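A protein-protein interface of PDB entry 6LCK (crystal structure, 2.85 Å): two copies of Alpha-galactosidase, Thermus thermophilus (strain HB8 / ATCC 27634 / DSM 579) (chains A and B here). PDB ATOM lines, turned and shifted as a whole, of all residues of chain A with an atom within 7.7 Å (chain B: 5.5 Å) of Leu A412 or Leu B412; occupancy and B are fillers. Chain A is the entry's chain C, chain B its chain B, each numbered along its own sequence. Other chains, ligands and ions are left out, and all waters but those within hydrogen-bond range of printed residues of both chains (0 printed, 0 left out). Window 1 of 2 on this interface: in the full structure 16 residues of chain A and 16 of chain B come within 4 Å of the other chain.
Pro A361 touches Leu B412. Leu B412 touches Phe A410 (CD2 to C, 3.6 Å). Phe A410 touches Leu B413. Asn A411 touches Asn B411. Asn A411 touches Leu B412. Leu A412 touches Pro B361. Leu A412 touches Phe B410 (CD2 to C, 3.4 Å). CD2 of Leu A412 touches N of Asn B411, at 3.5 Å. Leu B412 touches Leu A412. O of Leu A413 touches CE1 of Phe B410, 3.3 Å away.
Printed residues of chain B that touch a printed residue of chain A: Pro B361, Thr B408, Phe B410, Asn B411, Leu B412 and Leu B413. Among the printed residues, 15 pairs touch across the chains.
The guanidinium group of Arg A409 is in hydrogen-bond range of the side-chain hydroxyl of Thr B408. The backbone carbonyl oxygen of Thr B408 sits at hydrogen-bond distance from the backbone NH of Phe A410 (2.8 Å). The backbone carbonyl oxygen (O) of Thr A408 lies within hydrogen-bond range of the backbone NH (N) of Phe B410 (2.9 Å). The backbone carbonyl oxygen of Asn A411 lies close to the backbone NH of Phe B410 (3.3 Å). N of Phe A410 sits close to O of Asn B411 (3.5 Å).
Printed residues of chain B within 4 Å of Pro A361: Leu B412 (3.8 Å). Tyr A362 touches none of the printed residues of chain B. Of the printed residues of chain B, Phe A410 touches Thr B408, Asn B411, Leu B412 and Leu B413. Leu A412 touches just these residues of chain B: Pro B361, Phe B410, Asn B411 and Leu B412. Of the printed residues of chain A, Leu B412 touches Pro A361, Phe A410, Asn A411 and Leu A412. Glu B417 touches none of the printed residues of chain A. The nearest residue of chain B that does not touch Leu A412 is Tyr B362 (4.3 Å). The nearest printed residue of chain B that does not touch Pro A361 is Asn B411 (7.3 Å).
Thr A408 touches Phe B410, and with the chains exchanged Phe A410 touches Thr B408. Phe A410 touches Asn B411, and with the chains exchanged Asn A411 touches Phe B410. Asn A411 touches Leu B412, and with the chains exchanged Leu A412 touches Asn B411. Leu B412 touches its own counterpart, Leu A412. Of the 15 pairs that touch across the chains among the printed residues, 14 have their exchanged pair printed and touching as well.
The backbone NH (N) of Leu B413 sits at hydrogen-bond distance from the side-chain amide oxygen (OD1) of Asn B411 (2.8 Å). The backbone carbonyl oxygen of Pro A361 sits close to the side-chain amide oxygen of Asn A411, at 3.3 Å. N of Leu A412 sits at hydrogen-bond distance from O of Pro A361 (2.8 Å). NE of Arg A407 lies close to O of Arg A409 (3.1 Å). O of Phe A410 lies within hydrogen-bond range of NH2 of Arg A407. The backbone carbonyl oxygen (O) of Arg A407 is in hydrogen-bond range of the side-chain amide nitrogen (ND2) of Asn A411, at 3.1 Å.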
ATOM      1  N   TYR A 170      21.300  -0.353   8.687  1.00  0.00           N
ATOM      2  CA  TYR A 170      21.334  -0.455   7.224  1.00  0.00           C
ATOM      3  C   TYR A 170      21.728   0.921   6.686  1.00  0.00           C
ATOM      4  O   TYR A 170      22.653   1.539   7.231  1.00  0.00           O
ATOM      5  CB  TYR A 170      20.004  -1.026   6.732  1.00  0.00           C
ATOM      6  CG  TYR A 170      19.879  -2.464   7.168  1.00  0.00           C
ATOM      7  CD1 TYR A 170      20.354  -3.494   6.368  1.00  0.00           C
ATOM      8  CD2 TYR A 170      19.367  -2.790   8.420  1.00  0.00           C
ATOM      9  CE1 TYR A 170      20.274  -4.819   6.781  1.00  0.00           C
ATOM     10  CE2 TYR A 170      19.296  -4.100   8.842  1.00  0.00           C
ATOM     11  CZ  TYR A 170      19.751  -5.121   8.017  1.00  0.00           C
ATOM     12  OH  TYR A 170      19.693  -6.443   8.438  1.00  0.00           O
ATOM     13  N   ARG A 172      20.159   3.770   6.889  1.00  0.00           N
ATOM     14  CA  ARG A 172      19.637   4.918   7.641  1.00  0.00           C
ATOM     15  C   ARG A 172      20.592   5.234   8.791  1.00  0.00           C
ATOM     16  O   ARG A 172      20.295   5.040   9.973  1.00  0.00           O
ATOM     17  CB  ARG A 172      18.222   4.649   8.144  1.00  0.00           C
ATOM     18  CG  ARG A 172      17.319   3.867   7.197  1.00  0.00           C
ATOM     19  CD  ARG A 172      16.195   3.138   7.959  1.00  0.00           C
ATOM     20  NE  ARG A 172      16.551   1.780   8.422  1.00  0.00           N
ATOM     21  CZ  ARG A 172      16.495   1.367   9.696  1.00  0.00           C
ATOM     22  NH1 ARG A 172      16.094   2.199  10.657  1.00  0.00           N
ATOM     23  NH2 ARG A 172      16.836   0.118  10.019  1.00  0.00           N
ATOM     24  N   ALA A 360      21.477 -12.172   8.449  1.00  0.00           N
ATOM     25  CA  ALA A 360      20.293 -11.338   8.518  1.00  0.00           C
ATOM     26  C   ALA A 360      19.641 -11.613   9.855  1.00  0.00           C
ATOM     27  O   ALA A 360      19.980 -12.595  10.528  1.00  0.00           O
ATOM     28  CB  ALA A 360      19.339 -11.631   7.357  1.00  0.00           C
ATOM     29  N   PRO A 361      18.733 -10.759  10.290  1.00  0.00           N
ATOM     30  CA  PRO A 361      18.046 -11.049  11.557  1.00  0.00           C
ATOM     31  C   PRO A 361      16.953 -12.105  11.400  1.00  0.00           C
ATOM     32  O   PRO A 361      15.861 -11.989  11.961  1.00  0.00           O
ATOM     33  CB  PRO A 361      17.498  -9.680  11.984  1.00  0.00           C
ATOM     34  CG  PRO A 361      17.396  -8.896  10.716  1.00  0.00           C
ATOM     35  CD  PRO A 361      18.511  -9.376   9.838  1.00  0.00           C
ATOM     36  N   TYR A 362      17.250 -13.168  10.660  1.00  0.00           N
ATOM     37  CA  TYR A 362      16.292 -14.242  10.459  1.00  0.00           C
ATOM     38  C   TYR A 362      17.038 -15.414   9.838  1.00  0.00           C
ATOM     39  O   TYR A 362      18.081 -15.244   9.194  1.00  0.00           O
ATOM     40  CB  TYR A 362      15.095 -13.783   9.603  1.00  0.00           C
ATOM     41  CG  TYR A 362      15.480 -13.046   8.341  1.00  0.00           C
ATOM     42  CD1 TYR A 362      15.791 -13.750   7.199  1.00  0.00           C
ATOM     43  CD2 TYR A 362      15.551 -11.653   8.293  1.00  0.00           C
ATOM     44  CE1 TYR A 362      16.149 -13.111   6.041  1.00  0.00           C
ATOM     45  CE2 TYR A 362      15.923 -10.995   7.122  1.00  0.00           C
ATOM     46  CZ  TYR A 362      16.216 -11.744   5.995  1.00  0.00           C
ATOM     47  OH  TYR A 362      16.590 -11.179   4.792  1.00  0.00           O
ATOM     48  N   TRP A 363      16.497 -16.610  10.070  1.00  0.00           N
ATOM     49  CA  TRP A 363      17.136 -17.840   9.616  1.00  0.00           C
ATOM     50  C   TRP A 363      17.154 -17.940   8.088  1.00  0.00           C
ATOM     51  O   TRP A 363      18.211 -18.124   7.474  1.00  0.00           O
ATOM     52  CB  TRP A 363      16.409 -19.035  10.237  1.00  0.00           C
ATOM     53  CG  TRP A 363      16.992 -20.362   9.903  1.00  0.00           C
ATOM     54  CD1 TRP A 363      16.385 -21.358   9.212  1.00  0.00           C
ATOM     55  CD2 TRP A 363      18.291 -20.852  10.273  1.00  0.00           C
ATOM     56  NE1 TRP A 363      17.225 -22.444   9.117  1.00  0.00           N
ATOM     57  CE2 TRP A 363      18.400 -22.159   9.762  1.00  0.00           C
ATOM     58  CE3 TRP A 363      19.370 -20.314  10.987  1.00  0.00           C
ATOM     59  CZ2 TRP A 363      19.551 -22.934   9.932  1.00  0.00           C
ATOM     60  CZ3 TRP A 363      20.511 -21.085  11.164  1.00  0.00           C
ATOM     61  CH2 TRP A 363      20.594 -22.378  10.637  1.00  0.00           C
ATOM     62  N   TYR A 405      25.263 -11.813  15.947  1.00  0.00           N
ATOM     63  CA  TYR A 405      24.163 -11.179  16.661  1.00  0.00           C
ATOM     64  C   TYR A 405      24.192 -11.609  18.122  1.00  0.00           C
ATOM     65  O   TYR A 405      24.421 -12.788  18.430  1.00  0.00           O
ATOM     66  CB  TYR A 405      22.810 -11.544  16.045  1.00  0.00           C
ATOM     67  CG  TYR A 405      22.511 -10.904  14.712  1.00  0.00           C
ATOM     68  CD1 TYR A 405      22.888 -11.519  13.527  1.00  0.00           C
ATOM     69  CD2 TYR A 405      21.829  -9.691  14.632  1.00  0.00           C
ATOM     70  CE1 TYR A 405      22.610 -10.936  12.299  1.00  0.00           C
ATOM     71  CE2 TYR A 405      21.542  -9.102  13.409  1.00  0.00           C
ATOM     72  CZ  TYR A 405      21.939  -9.732  12.254  1.00  0.00           C
ATOM     73  OH  TYR A 405      21.652  -9.163  11.047  1.00  0.00           O
ATOM     74  N   ARG A 407      21.856  -9.294  20.167  1.00  0.00           N
ATOM     75  CA  ARG A 407      20.555  -8.764  20.522  1.00  0.00           C
ATOM     76  C   ARG A 407      19.454  -9.771  20.195  1.00  0.00           C
ATOM     77  O   ARG A 407      19.585 -10.605  19.298  1.00  0.00           O
ATOM     78  CB  ARG A 407      20.304  -7.452  19.793  1.00  0.00           C
ATOM     79  CG  ARG A 407      20.054  -7.624  18.321  1.00  0.00           C
ATOM     80  CD  ARG A 407      19.917  -6.293  17.650  1.00  0.00           C
ATOM     81  NE  ARG A 407      19.348  -6.395  16.312  1.00  0.00           N
ATOM     82  CZ  ARG A 407      20.039  -6.233  15.185  1.00  0.00           C
ATOM     83  NH1 ARG A 407      21.337  -5.983  15.221  1.00  0.00           N
ATOM     84  NH2 ARG A 407      19.426  -6.324  14.013  1.00  0.00           N
ATOM     85  N   THR A 408      18.379  -9.720  20.984  1.00  0.00           N
ATOM     86  CA  THR A 408      17.100 -10.290  20.597  1.00  0.00           C
ATOM     87  C   THR A 408      16.084  -9.228  20.205  1.00  0.00           C
ATOM     88  O   THR A 408      15.109  -9.543  19.519  1.00  0.00           O
ATOM     89  CB  THR A 408      16.511 -11.143  21.732  1.00  0.00           C
ATOM     90  OG1 THR A 408      16.439 -10.364  22.931  1.00  0.00           O
ATOM     91  CG2 THR A 408      17.361 -12.368  21.971  1.00  0.00           C
ATOM     92  N   ARG A 409      16.275  -7.993  20.626  1.00  0.00           N
ATOM     93  CA  ARG A 409      15.469  -6.920  20.083  1.00  0.00           C
ATOM     94  C   ARG A 409      15.794  -6.740  18.599  1.00  0.00           C
ATOM     95  O   ARG A 409      16.946  -6.876  18.180  1.00  0.00           O
ATOM     96  CB  ARG A 409      15.719  -5.637  20.884  1.00  0.00           C
ATOM     97  CG  ARG A 409      15.483  -5.836  22.392  1.00  0.00           C
ATOM     98  CD  ARG A 409      15.195  -4.540  23.180  1.00  0.00           C
ATOM     99  NE  ARG A 409      14.726  -3.446  22.340  1.00  0.00           N
ATOM    100  CZ  ARG A 409      14.882  -2.158  22.639  1.00  0.00           C
ATOM    101  NH1 ARG A 409      15.509  -1.813  23.758  1.00  0.00           N
ATOM    102  NH2 ARG A 409      14.437  -1.214  21.808  1.00  0.00           N
ATOM    103  N   PHE A 410      14.764  -6.468  17.799  1.00  0.00           N
ATOM    104  CA  PHE A 410      14.919  -6.189  16.375  1.00  0.00           C
ATOM    105  C   PHE A 410      15.712  -7.294  15.697  1.00  0.00           C
ATOM    106  O   PHE A 410      16.646  -7.045  14.933  1.00  0.00           O
ATOM    107  CB  PHE A 410      15.559  -4.822  16.152  1.00  0.00           C
ATOM    108  CG  PHE A 410      14.777  -3.682  16.764  1.00  0.00           C
ATOM    109  CD1 PHE A 410      13.538  -3.319  16.259  1.00  0.00           C
ATOM    110  CD2 PHE A 410      15.273  -2.985  17.854  1.00  0.00           C
ATOM    111  CE1 PHE A 410      12.823  -2.275  16.829  1.00  0.00           C
ATOM    112  CE2 PHE A 410      14.564  -1.948  18.414  1.00  0.00           C
ATOM    113  CZ  PHE A 410      13.341  -1.596  17.906  1.00  0.00           C
ATOM    114  N   ASN A 411      15.320  -8.535  15.999  1.00  0.00           N
ATOM    115  CA  ASN A 411      16.003  -9.720  15.504  1.00  0.00           C
ATOM    116  C   ASN A 411      15.076 -10.913  15.682  1.00  0.00           C
ATOM    117  O   ASN A 411      14.507 -11.090  16.763  1.00  0.00           O
ATOM    118  CB  ASN A 411      17.322  -9.933  16.252  1.00  0.00           C
ATOM    119  CG  ASN A 411      18.124 -11.076  15.698  1.00  0.00           C
ATOM    120  OD1 ASN A 411      17.741 -11.708  14.719  1.00  0.00           O
ATOM    121  ND2 ASN A 411      19.259 -11.348  16.320  1.00  0.00           N
ATOM    122  N   LEU A 412      14.926 -11.726  14.623  1.00  0.00           N
ATOM    123  CA  LEU A 412      14.031 -12.890  14.617  1.00  0.00           C
ATOM    124  C   LEU A 412      14.756 -14.205  14.888  1.00  0.00           C
ATOM    125  O   LEU A 412      14.096 -15.239  15.064  1.00  0.00           O
ATOM    126  CB  LEU A 412      13.267 -13.004  13.277  1.00  0.00           C
ATOM    127  CG  LEU A 412      12.280 -11.902  12.879  1.00  0.00           C
ATOM    128  CD1 LEU A 412      11.428 -12.317  11.703  1.00  0.00           C
ATOM    129  CD2 LEU A 412      11.423 -11.490  14.081  1.00  0.00           C
ATOM    130  N   LEU A 413      16.086 -14.193  14.926  1.00  0.00           N
ATOM    131  CA  LEU A 413      16.840 -15.399  15.215  1.00  0.00           C
ATOM    132  C   LEU A 413      16.515 -15.927  16.610  1.00  0.00           C
ATOM    133  O   LEU A 413      16.294 -15.164  17.558  1.00  0.00           O
ATOM    134  CB  LEU A 413      18.333 -15.109  15.104  1.00  0.00           C
ATOM    135  CG  LEU A 413      18.772 -14.776  13.694  1.00  0.00           C
ATOM    136  CD1 LEU A 413      20.165 -14.203  13.709  1.00  0.00           C
ATOM    137  CD2 LEU A 413      18.704 -16.026  12.843  1.00  0.00           C
ATOM    138  N   SER A 414      16.487 -17.245  16.735  1.00  0.00           N
ATOM    139  CA  SER A 414      16.423 -17.859  18.048  1.00  0.00           C
ATOM    140  C   SER A 414      17.785 -17.793  18.716  1.00  0.00           C
ATOM    141  O   SER A 414      18.804 -17.570  18.059  1.00  0.00           O
ATOM    142  CB  SER A 414      15.998 -19.317  17.936  1.00  0.00           C
ATOM    143  OG  SER A 414      17.037 -20.078  17.345  1.00  0.00           O
ATOM    144  N   PRO A 415      17.829 -17.975  20.033  1.00  0.00           N
ATOM    145  CA  PRO A 415      19.132 -18.133  20.702  1.00  0.00           C
ATOM    146  C   PRO A 415      19.964 -19.298  20.184  1.00  0.00           C
ATOM    147  O   PRO A 415      21.182 -19.146  20.018  1.00  0.00           O
ATOM    148  CB  PRO A 415      18.725 -18.316  22.163  1.00  0.00           C
ATOM    149  CG  PRO A 415      17.505 -17.418  22.277  1.00  0.00           C
ATOM    150  CD  PRO A 415      16.754 -17.629  20.979  1.00  0.00           C
ATOM    151  N   GLU A 417      20.058 -20.469  17.213  1.00  0.00           N
ATOM    152  CA  GLU A 417      20.592 -20.068  15.912  1.00  0.00           C
ATOM    153  C   GLU A 417      21.730 -19.064  16.068  1.00  0.00           C
ATOM    154  O   GLU A 417      22.739 -19.131  15.353  1.00  0.00           O
ATOM    155  CB  GLU A 417      19.469 -19.486  15.045  1.00  0.00           C
ATOM    156  CG  GLU A 417      18.432 -20.506  14.531  1.00  0.00           C
ATOM    157  CD  GLU A 417      17.080 -19.858  14.271  1.00  0.00           C
ATOM    158  OE1 GLU A 417      16.935 -18.667  14.616  1.00  0.00           O
ATOM    159  OE2 GLU A 417      16.165 -20.525  13.740  1.00  0.00           O
ATOM    160  N   MET A 418      21.592 -18.135  17.010  1.00  0.00           N
ATOM    161  CA  MET A 418      22.621 -17.125  17.208  1.00  0.00           C
ATOM    162  C   MET A 418      23.948 -17.750  17.609  1.00  0.00           C
ATOM    163  O   MET A 418      25.010 -17.239  17.233  1.00  0.00           O
ATOM    164  CB  MET A 418      22.169 -16.121  18.268  1.00  0.00           C
ATOM    165  CG  MET A 418      21.262 -15.062  17.711  1.00  0.00           C
ATOM    166  SD  MET A 418      20.849 -13.764  18.883  1.00  0.00           S
ATOM    167  CE  MET A 418      19.170 -14.197  19.341  1.00  0.00           C
ATOM    168  N   PRO B 361       6.171 -10.181  11.919  1.00  0.00           N
ATOM    169  CA  PRO B 361       7.147  -9.322  12.603  1.00  0.00           C
ATOM    170  C   PRO B 361       8.042  -8.563  11.622  1.00  0.00           C
ATOM    171  O   PRO B 361       9.246  -8.425  11.860  1.00  0.00           O
ATOM    172  CB  PRO B 361       7.942 -10.316  13.454  1.00  0.00           C
ATOM    173  CG  PRO B 361       7.830 -11.613  12.702  1.00  0.00           C
ATOM    174  CD  PRO B 361       6.453 -11.611  12.132  1.00  0.00           C
ATOM    175  N   TYR B 362       7.485  -8.072  10.516  1.00  0.00           N
ATOM    176  CA  TYR B 362       8.263  -7.297   9.560  1.00  0.00           C
ATOM    177  C   TYR B 362       7.291  -6.535   8.676  1.00  0.00           C
ATOM    178  O   TYR B 362       6.116  -6.889   8.562  1.00  0.00           O
ATOM    179  CB  TYR B 362       9.209  -8.170   8.717  1.00  0.00           C
ATOM    180  CG  TYR B 362       8.584  -9.433   8.143  1.00  0.00           C
ATOM    181  CD1 TYR B 362       7.701  -9.372   7.075  1.00  0.00           C
ATOM    182  CD2 TYR B 362       8.885 -10.687   8.662  1.00  0.00           C
ATOM    183  CE1 TYR B 362       7.129 -10.511   6.555  1.00  0.00           C
ATOM    184  CE2 TYR B 362       8.320 -11.829   8.140  1.00  0.00           C
ATOM    185  CZ  TYR B 362       7.437 -11.739   7.086  1.00  0.00           C
ATOM    186  OH  TYR B 362       6.849 -12.873   6.546  1.00  0.00           O
ATOM    187  N   THR B 408       9.563  -5.608  21.169  1.00  0.00           N
ATOM    188  CA  THR B 408      10.612  -5.390  20.202  1.00  0.00           C
ATOM    189  C   THR B 408      11.585  -6.556  20.129  1.00  0.00           C
ATOM    190  O   THR B 408      12.322  -6.667  19.150  1.00  0.00           O
ATOM    191  CB  THR B 408      11.341  -4.086  20.520  1.00  0.00           C
ATOM    192  OG1 THR B 408      11.684  -4.058  21.910  1.00  0.00           O
ATOM    193  CG2 THR B 408      10.419  -2.935  20.220  1.00  0.00           C
ATOM    194  N   PHE B 410      12.367 -10.227  19.148  1.00  0.00           N
ATOM    195  CA  PHE B 410      11.803 -11.189  18.200  1.00  0.00           C
ATOM    196  C   PHE B 410      10.751 -10.525  17.312  1.00  0.00           C
ATOM    197  O   PHE B 410       9.689 -11.092  17.034  1.00  0.00           O
ATOM    198  CB  PHE B 410      11.250 -12.410  18.937  1.00  0.00           C
ATOM    199  CG  PHE B 410      12.268 -13.067  19.821  1.00  0.00           C
ATOM    200  CD1 PHE B 410      13.397 -13.666  19.268  1.00  0.00           C
ATOM    201  CD2 PHE B 410      12.127 -13.053  21.203  1.00  0.00           C
ATOM    202  CE1 PHE B 410      14.360 -14.257  20.080  1.00  0.00           C
ATOM    203  CE2 PHE B 410      13.087 -13.638  22.017  1.00  0.00           C
ATOM    204  CZ  PHE B 410      14.205 -14.240  21.455  1.00  0.00           C
ATOM    205  N   ASN B 411      11.075  -9.311  16.856  1.00  0.00           N
ATOM    206  CA  ASN B 411      10.213  -8.502  16.008  1.00  0.00           C
ATOM    207  C   ASN B 411      11.096  -7.512  15.250  1.00  0.00           C
ATOM    208  O   ASN B 411      11.916  -6.828  15.867  1.00  0.00           O
ATOM    209  CB  ASN B 411       9.159  -7.783  16.861  1.00  0.00           C
ATOM    210  CG  ASN B 411       8.186  -6.979  16.037  1.00  0.00           C
ATOM    211  OD1 ASN B 411       8.234  -6.995  14.808  1.00  0.00           O
ATOM    212  ND2 ASN B 411       7.286  -6.268  16.709  1.00  0.00           N
ATOM    213  N   LEU B 412      10.938  -7.440  13.921  1.00  0.00           N
ATOM    214  CA  LEU B 412      11.663  -6.468  13.106  1.00  0.00           C
ATOM    215  C   LEU B 412      10.905  -5.161  12.917  1.00  0.00           C
ATOM    216  O   LEU B 412      11.438  -4.234  12.296  1.00  0.00           O
ATOM    217  CB  LEU B 412      11.997  -7.046  11.726  1.00  0.00           C
ATOM    218  CG  LEU B 412      12.855  -8.318  11.644  1.00  0.00           C
ATOM    219  CD1 LEU B 412      13.330  -8.549  10.203  1.00  0.00           C
ATOM    220  CD2 LEU B 412      14.037  -8.289  12.630  1.00  0.00           C
ATOM    221  N   LEU B 413       9.682  -5.054  13.414  1.00  0.00           N
ATOM    222  CA  LEU B 413       8.891  -3.866  13.135  1.00  0.00           C
ATOM    223  C   LEU B 413       9.389  -2.659  13.920  1.00  0.00           C
ATOM    224  O   LEU B 413       9.922  -2.782  15.025  1.00  0.00           O
ATOM    225  CB  LEU B 413       7.438  -4.111  13.484  1.00  0.00           C
ATOM    226  CG  LEU B 413       6.715  -5.010  12.517  1.00  0.00           C
ATOM    227  CD1 LEU B 413       5.370  -5.353  13.174  1.00  0.00           C
ATOM    228  CD2 LEU B 413       6.542  -4.255  11.219  1.00  0.00           C
ATOM    229  N   SER B 414       9.189  -1.519  13.368  1.00  0.00           N
ATOM    230  CA  SER B 414       9.555  -0.289  14.059  1.00  0.00           C
ATOM    231  C   SER B 414       8.409   0.197  14.945  1.00  0.00           C
ATOM    232  O   SER B 414       7.239  -0.079  14.663  1.00  0.00           O
ATOM    233  CB  SER B 414       9.918   0.804  13.051  1.00  0.00           C
ATOM    234  OG  SER B 414       8.788   1.560  12.643  1.00  0.00           O
ATOM    235  N   GLU B 417       5.799   1.798  12.997  1.00  0.00           N
ATOM    236  CA  GLU B 417       5.034   0.801  12.260  1.00  0.00           C
ATOM    237  C   GLU B 417       4.025   0.110  13.173  1.00  0.00           C
ATOM    238  O   GLU B 417       2.834   0.019  12.850  1.00  0.00           O
ATOM    239  CB  GLU B 417       5.994  -0.200  11.626  1.00  0.00           C
ATOM    240  CG  GLU B 417       6.753   0.366  10.405  1.00  0.00           C
ATOM    241  CD  GLU B 417       7.937  -0.492   9.949  1.00  0.00           C
ATOM    242  OE1 GLU B 417       8.400  -1.392  10.695  1.00  0.00           O
ATOM    243  OE2 GLU B 417       8.405  -0.264   8.819  1.00  0.00           O
